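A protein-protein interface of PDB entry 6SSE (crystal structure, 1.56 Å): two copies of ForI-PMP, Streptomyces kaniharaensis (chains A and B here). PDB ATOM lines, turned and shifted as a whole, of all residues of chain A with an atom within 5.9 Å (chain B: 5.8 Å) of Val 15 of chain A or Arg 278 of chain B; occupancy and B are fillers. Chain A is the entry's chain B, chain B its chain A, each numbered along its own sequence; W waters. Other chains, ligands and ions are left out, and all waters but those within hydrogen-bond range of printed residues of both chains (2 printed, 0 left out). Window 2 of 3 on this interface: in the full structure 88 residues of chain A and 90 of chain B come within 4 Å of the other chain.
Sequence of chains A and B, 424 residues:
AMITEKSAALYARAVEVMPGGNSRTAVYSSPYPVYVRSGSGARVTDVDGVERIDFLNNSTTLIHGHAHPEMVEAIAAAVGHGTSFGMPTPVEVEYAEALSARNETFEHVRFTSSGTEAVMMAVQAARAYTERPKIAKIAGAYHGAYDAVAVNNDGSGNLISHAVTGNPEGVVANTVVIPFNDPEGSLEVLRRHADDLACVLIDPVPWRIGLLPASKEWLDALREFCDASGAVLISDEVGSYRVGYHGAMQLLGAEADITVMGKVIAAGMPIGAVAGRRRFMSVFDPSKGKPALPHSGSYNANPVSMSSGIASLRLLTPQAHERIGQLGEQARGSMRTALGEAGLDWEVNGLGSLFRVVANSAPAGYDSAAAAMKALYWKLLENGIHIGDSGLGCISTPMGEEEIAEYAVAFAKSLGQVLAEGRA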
ATOM      1  N   LEU A  10      -6.950  -1.984 -19.614  1.00  0.00           N
ATOM      2  CA  LEU A  10      -6.698  -1.303 -20.921  1.00  0.00           C
ATOM      3  C   LEU A  10      -5.672  -0.211 -20.727  1.00  0.00           C
ATOM      4  O   LEU A  10      -4.809  -0.067 -21.597  1.00  0.00           O
ATOM      5  CB  LEU A  10      -8.040  -0.750 -21.438  1.00  0.00           C
ATOM      6  CG  LEU A  10      -8.842  -1.806 -22.170  1.00  0.00           C
ATOM      7  CD1 LEU A  10     -10.291  -1.371 -22.392  1.00  0.00           C
ATOM      8  CD2 LEU A  10      -8.175  -2.238 -23.469  1.00  0.00           C
ATOM      9  N   TYR A  11      -5.754   0.591 -19.661  1.00  0.00           N
ATOM     10  CA  TYR A  11      -4.797   1.673 -19.429  1.00  0.00           C
ATOM     11  C   TYR A  11      -3.383   1.106 -19.275  1.00  0.00           C
ATOM     12  O   TYR A  11      -2.434   1.660 -19.830  1.00  0.00           O
ATOM     13  CB  TYR A  11      -5.195   2.524 -18.226  1.00  0.00           C
ATOM     14  CG  TYR A  11      -4.358   3.752 -18.121  1.00  0.00           C
ATOM     15  CD1 TYR A  11      -4.385   4.736 -19.108  1.00  0.00           C
ATOM     16  CD2 TYR A  11      -3.484   3.929 -17.061  1.00  0.00           C
ATOM     17  CE1 TYR A  11      -3.618   5.888 -19.012  1.00  0.00           C
ATOM     18  CE2 TYR A  11      -2.695   5.053 -16.969  1.00  0.00           C
ATOM     19  CZ  TYR A  11      -2.734   6.037 -17.958  1.00  0.00           C
ATOM     20  OH  TYR A  11      -1.924   7.146 -17.894  1.00  0.00           O
ATOM     21  N   ALA A  12      -3.234   0.006 -18.553  1.00  0.00           N
ATOM     22  CA  ALA A  12      -1.926  -0.664 -18.374  1.00  0.00           C
ATOM     23  C   ALA A  12      -1.308  -1.070 -19.723  1.00  0.00           C
ATOM     24  O   ALA A  12      -0.093  -0.991 -19.864  1.00  0.00           O
ATOM     25  CB  ALA A  12      -2.125  -1.858 -17.482  1.00  0.00           C
ATOM     26  N   ARG A  13      -2.115  -1.523 -20.650  1.00  0.00           N
ATOM     27  CA  ARG A  13      -1.647  -1.826 -22.031  1.00  0.00           C
ATOM     28  C   ARG A  13      -1.339  -0.492 -22.725  1.00  0.00           C
ATOM     29  O   ARG A  13      -0.296  -0.402 -23.427  1.00  0.00           O
ATOM     30  CB  ARG A  13      -2.722  -2.612 -22.783  1.00  0.00           C
ATOM     31  CG  ARG A  13      -2.826  -4.077 -22.366  1.00  0.00           C
ATOM     32  CD  ARG A  13      -4.106  -4.669 -22.878  1.00  0.00           C
ATOM     33  NE  ARG A  13      -4.139  -4.669 -24.348  1.00  0.00           N
ATOM     34  CZ  ARG A  13      -5.246  -4.854 -25.047  1.00  0.00           C
ATOM     35  NH1 ARG A  13      -6.380  -5.070 -24.419  1.00  0.00           N
ATOM     36  NH2 ARG A  13      -5.207  -4.843 -26.370  1.00  0.00           N
ATOM     37  N   ALA A  14      -2.221   0.492 -22.580  1.00  0.00           N
ATOM     38  CA  ALA A  14      -2.101   1.747 -23.344  1.00  0.00           C
ATOM     39  C   ALA A  14      -0.801   2.487 -23.018  1.00  0.00           C
ATOM     40  O   ALA A  14      -0.167   3.052 -23.939  1.00  0.00           O
ATOM     41  CB  ALA A  14      -3.284   2.613 -23.118  1.00  0.00           C
ATOM     42  N   VAL A  15      -0.380   2.522 -21.747  1.00  0.00           N
ATOM     43  CA  VAL A  15       0.845   3.273 -21.382  1.00  0.00           C
ATOM     44  C   VAL A  15       2.096   2.702 -22.060  1.00  0.00           C
ATOM     45  O   VAL A  15       3.091   3.413 -22.110  1.00  0.00           O
ATOM     46  CB  VAL A  15       1.008   3.344 -19.852  1.00  0.00           C
ATOM     47  CG1 VAL A  15      -0.081   4.151 -19.225  1.00  0.00           C
ATOM     48  CG2 VAL A  15       1.081   1.948 -19.247  1.00  0.00           C
ATOM     49  N   GLU A  16       2.086   1.443 -22.552  1.00  0.00           N
ATOM     50  CA  GLU A  16       3.255   0.845 -23.211  1.00  0.00           C
ATOM     51  C   GLU A  16       3.358   1.310 -24.665  1.00  0.00           C
ATOM     52  O   GLU A  16       4.485   1.201 -25.224  1.00  0.00           O
ATOM     53  CB  GLU A  16       3.203  -0.692 -23.186  1.00  0.00           C
ATOM     54  CG  GLU A  16       3.134  -1.263 -21.778  1.00  0.00           C
ATOM     55  CD  GLU A  16       4.326  -0.886 -20.916  1.00  0.00           C
ATOM     56  OE1 GLU A  16       5.430  -0.720 -21.485  1.00  0.00           O
ATOM     57  OE2 GLU A  16       4.118  -0.678 -19.680  1.00  0.00           O
ATOM     58  N   VAL A  17       2.251   1.835 -25.245  1.00  0.00           N
ATOM     59  CA  VAL A  17       2.248   2.121 -26.714  1.00  0.00           C
ATOM     60  C   VAL A  17       1.744   3.534 -27.059  1.00  0.00           C
ATOM     61  O   VAL A  17       1.804   3.864 -28.255  1.00  0.00           O
ATOM     62  CB  VAL A  17       1.443   1.073 -27.476  1.00  0.00           C
ATOM     63  CG1 VAL A  17       2.151  -0.295 -27.399  1.00  0.00           C
ATOM     64  CG2 VAL A  17       0.012   1.006 -26.970  1.00  0.00           C
ATOM     65  N   MET A  18       1.355   4.324 -26.064  1.00  0.00           N
ATOM     66  CA  MET A  18       0.941   5.734 -26.259  1.00  0.00           C
ATOM     67  C   MET A  18       1.524   6.557 -25.130  1.00  0.00           C
ATOM     68  O   MET A  18       1.725   6.038 -24.039  1.00  0.00           O
ATOM     69  CB  MET A  18      -0.571   5.904 -26.193  1.00  0.00           C
ATOM     70  CG  MET A  18      -1.377   5.094 -27.154  1.00  0.00           C
ATOM     71  SD  MET A  18      -3.126   5.527 -26.770  1.00  0.00           S
ATOM     72  CE  MET A  18      -3.944   4.876 -28.223  1.00  0.00           C
ATOM     73  N   PRO A  19       1.785   7.861 -25.335  1.00  0.00           N
ATOM     74  CA  PRO A  19       2.354   8.697 -24.270  1.00  0.00           C
ATOM     75  C   PRO A  19       1.335   8.892 -23.134  1.00  0.00           C
ATOM     76  O   PRO A  19       0.281   9.532 -23.300  1.00  0.00           O
ATOM     77  CB  PRO A  19       2.697  10.020 -24.923  1.00  0.00           C
ATOM     78  CG  PRO A  19       2.323   9.888 -26.380  1.00  0.00           C
ATOM     79  CD  PRO A  19       1.631   8.570 -26.606  1.00  0.00           C
ATOM     80  N   GLY A  20       1.689   8.416 -21.962  1.00  0.00           N
ATOM     81  CA  GLY A  20       0.774   8.368 -20.809  1.00  0.00           C
ATOM     82  C   GLY A  20      -0.502   7.618 -21.142  1.00  0.00           C
ATOM     83  O   GLY A  20      -1.506   7.841 -20.461  1.00  0.00           O
ATOM     84  N   GLY A  21      -0.461   6.683 -22.116  1.00  0.00           N
ATOM     85  CA  GLY A  21      -1.624   5.856 -22.453  1.00  0.00           C
ATOM     86  C   GLY A  21      -2.708   6.672 -23.107  1.00  0.00           C
ATOM     87  O   GLY A  21      -3.861   6.288 -23.069  1.00  0.00           O
ATOM     88  N   GLU B 107       7.855   3.384 -30.578  1.00  0.00           N
ATOM     89  CA  GLU B 107       7.655   2.987 -29.165  1.00  0.00           C
ATOM     90  C   GLU B 107       6.335   3.508 -28.656  1.00  0.00           C
ATOM     91  O   GLU B 107       5.579   2.759 -28.036  1.00  0.00           O
ATOM     92  CB  GLU B 107       8.794   3.545 -28.315  1.00  0.00           C
ATOM     93  CG  GLU B 107      10.123   2.888 -28.651  1.00  0.00           C
ATOM     94  CD  GLU B 107      11.311   3.390 -27.865  1.00  0.00           C
ATOM     95  OE1 GLU B 107      11.207   4.434 -27.164  1.00  0.00           O
ATOM     96  OE2 GLU B 107      12.347   2.713 -27.943  1.00  0.00           O
ATOM     97  N   HIS B 108       6.036   4.774 -28.917  1.00  0.00           N
ATOM     98  CA  HIS B 108       4.765   5.410 -28.530  1.00  0.00           C
ATOM     99  C   HIS B 108       4.139   6.084 -29.744  1.00  0.00           C
ATOM    100  O   HIS B 108       4.891   6.698 -30.532  1.00  0.00           O
ATOM    101  CB  HIS B 108       4.986   6.492 -27.466  1.00  0.00           C
ATOM    102  CG  HIS B 108       5.030   5.931 -26.084  1.00  0.00           C
ATOM    103  ND1 HIS B 108       5.258   6.756 -24.992  1.00  0.00           N
ATOM    104  CD2 HIS B 108       4.919   4.671 -25.613  1.00  0.00           C
ATOM    105  CE1 HIS B 108       5.176   6.029 -23.898  1.00  0.00           C
ATOM    106  NE2 HIS B 108       4.981   4.762 -24.233  1.00  0.00           N
ATOM    107  N   GLY B 276       7.117   7.447 -32.341  1.00  0.00           N
ATOM    108  CA  GLY B 276       8.564   7.602 -32.158  1.00  0.00           C
ATOM    109  C   GLY B 276       9.037   7.147 -30.799  1.00  0.00           C
ATOM    110  O   GLY B 276       8.272   6.553 -30.027  1.00  0.00           O
ATOM    111  N   ARG B 277      10.296   7.473 -30.501  1.00  0.00           N
ATOM    112  CA  ARG B 277      10.895   7.029 -29.238  1.00  0.00           C
ATOM    113  C   ARG B 277      10.141   7.727 -28.110  1.00  0.00           C
ATOM    114  O   ARG B 277       9.692   8.888 -28.269  1.00  0.00           O
ATOM    115  CB  ARG B 277      12.397   7.375 -29.190  1.00  0.00           C
ATOM    116  CG  ARG B 277      13.236   6.764 -30.293  1.00  0.00           C
ATOM    117  CD  ARG B 277      13.295   5.247 -30.208  1.00  0.00           C
ATOM    118  NE  ARG B 277      14.235   4.686 -31.177  1.00  0.00           N
ATOM    119  CZ  ARG B 277      14.677   3.420 -31.139  1.00  0.00           C
ATOM    120  NH1 ARG B 277      14.201   2.571 -30.246  1.00  0.00           N
ATOM    121  NH2 ARG B 277      15.547   3.005 -32.044  1.00  0.00           N
ATOM    122  N   ARG B 278      10.024   7.062 -26.965  1.00  0.00           N
ATOM    123  CA  ARG B 278       9.257   7.557 -25.799  1.00  0.00           C
ATOM    124  C   ARG B 278       9.680   8.993 -25.455  1.00  0.00           C
ATOM    125  O   ARG B 278       8.784   9.805 -25.186  1.00  0.00           O
ATOM    126  CB  ARG B 278       9.329   6.581 -24.617  1.00  0.00           C
ATOM    127  CG  ARG B 278       8.741   5.203 -24.909  1.00  0.00           C
ATOM    128  CD  ARG B 278       8.892   4.084 -23.874  1.00  0.00           C
ATOM    129  NE  ARG B 278       7.742   3.961 -22.992  1.00  0.00           N
ATOM    130  CZ  ARG B 278       6.973   2.878 -22.811  1.00  0.00           C
ATOM    131  NH1 ARG B 278       5.957   2.960 -21.969  1.00  0.00           N
ATOM    132  NH2 ARG B 278       7.197   1.742 -23.463  1.00  0.00           N
ATOM    133  N   ARG B 279      10.985   9.310 -25.444  1.00  0.00           N
ATOM    134  CA  ARG B 279      11.447  10.642 -24.958  1.00  0.00           C
ATOM    135  C   ARG B 279      10.863  11.759 -25.835  1.00  0.00           C
ATOM    136  O   ARG B 279      10.440  12.775 -25.279  1.00  0.00           O
ATOM    137  CB  ARG B 279      12.968  10.784 -24.891  1.00  0.00           C
ATOM    138  CG  ARG B 279      13.728  10.623 -26.197  1.00  0.00           C
ATOM    139  CD  ARG B 279      15.234  10.403 -25.870  1.00  0.00           C
ATOM    140  NE  ARG B 279      16.027  10.093 -27.034  1.00  0.00           N
ATOM    141  CZ  ARG B 279      16.041   8.912 -27.647  1.00  0.00           C
ATOM    142  NH1 ARG B 279      15.334   7.903 -27.176  1.00  0.00           N
ATOM    143  NH2 ARG B 279      16.741   8.765 -28.736  1.00  0.00           N
ATOM    144  N   PHE B 280      10.805  11.584 -27.156  1.00  0.00           N
ATOM    145  CA  PHE B 280      10.295  12.661 -28.063  1.00  0.00           C
ATOM    146  C   PHE B 280       8.765  12.751 -27.941  1.00  0.00           C
ATOM    147  O   PHE B 280       8.212  13.856 -27.898  1.00  0.00           O
ATOM    148  CB  PHE B 280      10.686  12.380 -29.507  1.00  0.00           C
ATOM    149  CG  PHE B 280      12.165  12.200 -29.708  1.00  0.00           C
ATOM    150  CD1 PHE B 280      13.026  13.255 -29.491  1.00  0.00           C
ATOM    151  CD2 PHE B 280      12.690  10.964 -30.036  1.00  0.00           C
ATOM    152  CE1 PHE B 280      14.393  13.091 -29.660  1.00  0.00           C
ATOM    153  CE2 PHE B 280      14.063  10.784 -30.150  1.00  0.00           C
ATOM    154  CZ  PHE B 280      14.909  11.840 -29.960  1.00  0.00           C
ATOM    155  N   MET B 281       8.104  11.636 -27.716  1.00  0.00           N
ATOM    156  CA  MET B 281       6.630  11.558 -27.606  1.00  0.00           C
ATOM    157  C   MET B 281       6.193  12.017 -26.198  1.00  0.00           C
ATOM    158  O   MET B 281       5.009  12.280 -25.989  1.00  0.00           O
ATOM    159  CB  MET B 281       6.156  10.125 -27.894  1.00  0.00           C
ATOM    160  CG  MET B 281       6.500   9.641 -29.334  1.00  0.00           C
ATOM    161  SD  MET B 281       5.629  10.680 -30.596  1.00  0.00           S
ATOM    162  CE  MET B 281       3.949  10.228 -30.252  1.00  0.00           C
ATOM    163  N   SER B 282       7.106  12.113 -25.218  1.00  0.00           N
ATOM    164  CA  SER B 282       6.723  12.478 -23.818  1.00  0.00           C
ATOM    165  C   SER B 282       6.135  13.896 -23.727  1.00  0.00           C
ATOM    166  O   SER B 282       5.439  14.195 -22.716  1.00  0.00           O
ATOM    167  CB  SER B 282       7.896  12.334 -22.843  1.00  0.00           C
ATOM    168  OG  SER B 282       8.931  13.230 -23.130  1.00  0.00           O
ATOM    169  N   VAL B 283       6.377  14.778 -24.682  1.00  0.00           N
ATOM    170  CA  VAL B 283       5.752  16.139 -24.688  1.00  0.00           C
ATOM    171  C   VAL B 283       4.219  16.027 -24.674  1.00  0.00           C
ATOM    172  O   VAL B 283       3.545  16.916 -24.135  1.00  0.00           O
ATOM    173  CB  VAL B 283       6.232  17.022 -25.852  1.00  0.00           C
ATOM    174  CG1 VAL B 283       7.722  17.263 -25.741  1.00  0.00           C
ATOM    175  CG2 VAL B 283       5.868  16.453 -27.206  1.00  0.00           C
HETATM  176  O   HOH W   1       6.512  -1.324 -23.827  1.00  0.00           O
HETATM  177  O   HOH W   2       5.773   0.146 -27.779  1.00  0.00           O
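No position is printed for both chains.
Of the 10 pairs that touch across the chains among the printed residues, none has its exchanged pair printed and touching as well.
NE2 of His 108 of chain B sits at hydrogen-bond distance from O of Val 15 of chain A (3.1 Å).
The backbone carbonyl oxygen (O) of Val 15 of chain A is in hydrogen-bond range of the guanidinium group (NH1) of Arg 278 of chain B, 2.9 Å away.
NH2 of Arg 278 of chain B is in salt-bridge range of OE1 of Glu 16 of chain A (3.6 Å).
The backbone carbonyl oxygen of Glu 16 of chain A lies close to the backbone carbonyl oxygen of Glu 107 of chain B (3.4 Å).
Water W2 lies within hydrogen-bond range of O of Glu 107 of chain B and O of Glu 16 of chain A.
Water W1 lies within hydrogen-bond range of OE1 of Glu 16 of chain A (2.6 Å) and NH2 of Arg 278 of chain B (3.2 Å).
Printed residues of chain B within 4 Å of Val 15 of chain A: His 108 and Arg 278.
Printed residues of chain A within 4 Å of Glu 107 of chain B: Glu 16 and Val 17.
Printed residues of chain A within 4 Å of His 108 of chain B: Val 15, Glu 16, Val 17, Met 18 and Pro 19.
Arg 279 of chain B touches none of the printed residues of chain A.
Gly 21 of chain A touches none of the printed residues of chain B.
The nearest printed residue of chain B that does not touch Val 15 of chain A is Glu 107 of chain B (6.5 Å).
The nearest printed residue of chain A that does not touch Arg 278 of chain B is Val 17 of chain A (5.1 Å).
Printed residues of chain A that touch a printed residue of chain B: Val 15, Glu 16, Val 17, Met 18 and Pro 19.
Among the printed residues, 10 pairs touch across the chains.
Among the printed residues, Asp or Glu carboxylates within 4 Å of a Lys or Arg side-chain nitrogen of the other chain: Glu 16 of chain A with Arg 278 of chain B (3.6 Å).
N of Glu 107 of chain B sits at hydrogen-bond distance from O of Gly 276 of chain B, at 3.2 Å.
The guanidinium group (NH1) of Arg 277 of chain B is in salt-bridge range of the side-chain carboxylate (OE2) of Glu 107 of chain B, 3.0 Å away.
The side-chain carboxylate of Glu 107 of chain B lies within hydrogen-bond range of the backbone NH of Arg 278 of chain B, 2.9 Å away.
O of His 108 of chain B sits at hydrogen-bond distance from N of Gly 276 of chain B, at 3.0 Å.
The guanidinium group (NH1) of Arg 278 of chain B sits at hydrogen-bond distance from a ring nitrogen (NE2) of His 108 of chain B, 3.1 Å away.
Among the printed residues, pairs that only touch across the chains: Glu 16 of chain A with His 108 of chain B (3.5 Å), Val 17 of chain A with Glu 107 of chain B (3.6 Å), Val 17 of chain A with His 108 of chain B (3.4 Å), Met 18 of chain A with His 108 of chain B (3.5 Å), Pro 19 of chain A with His 108 of chain B (3.6 Å) and Pro 19 of chain A with Met 281 of chain B (3.4 Å).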
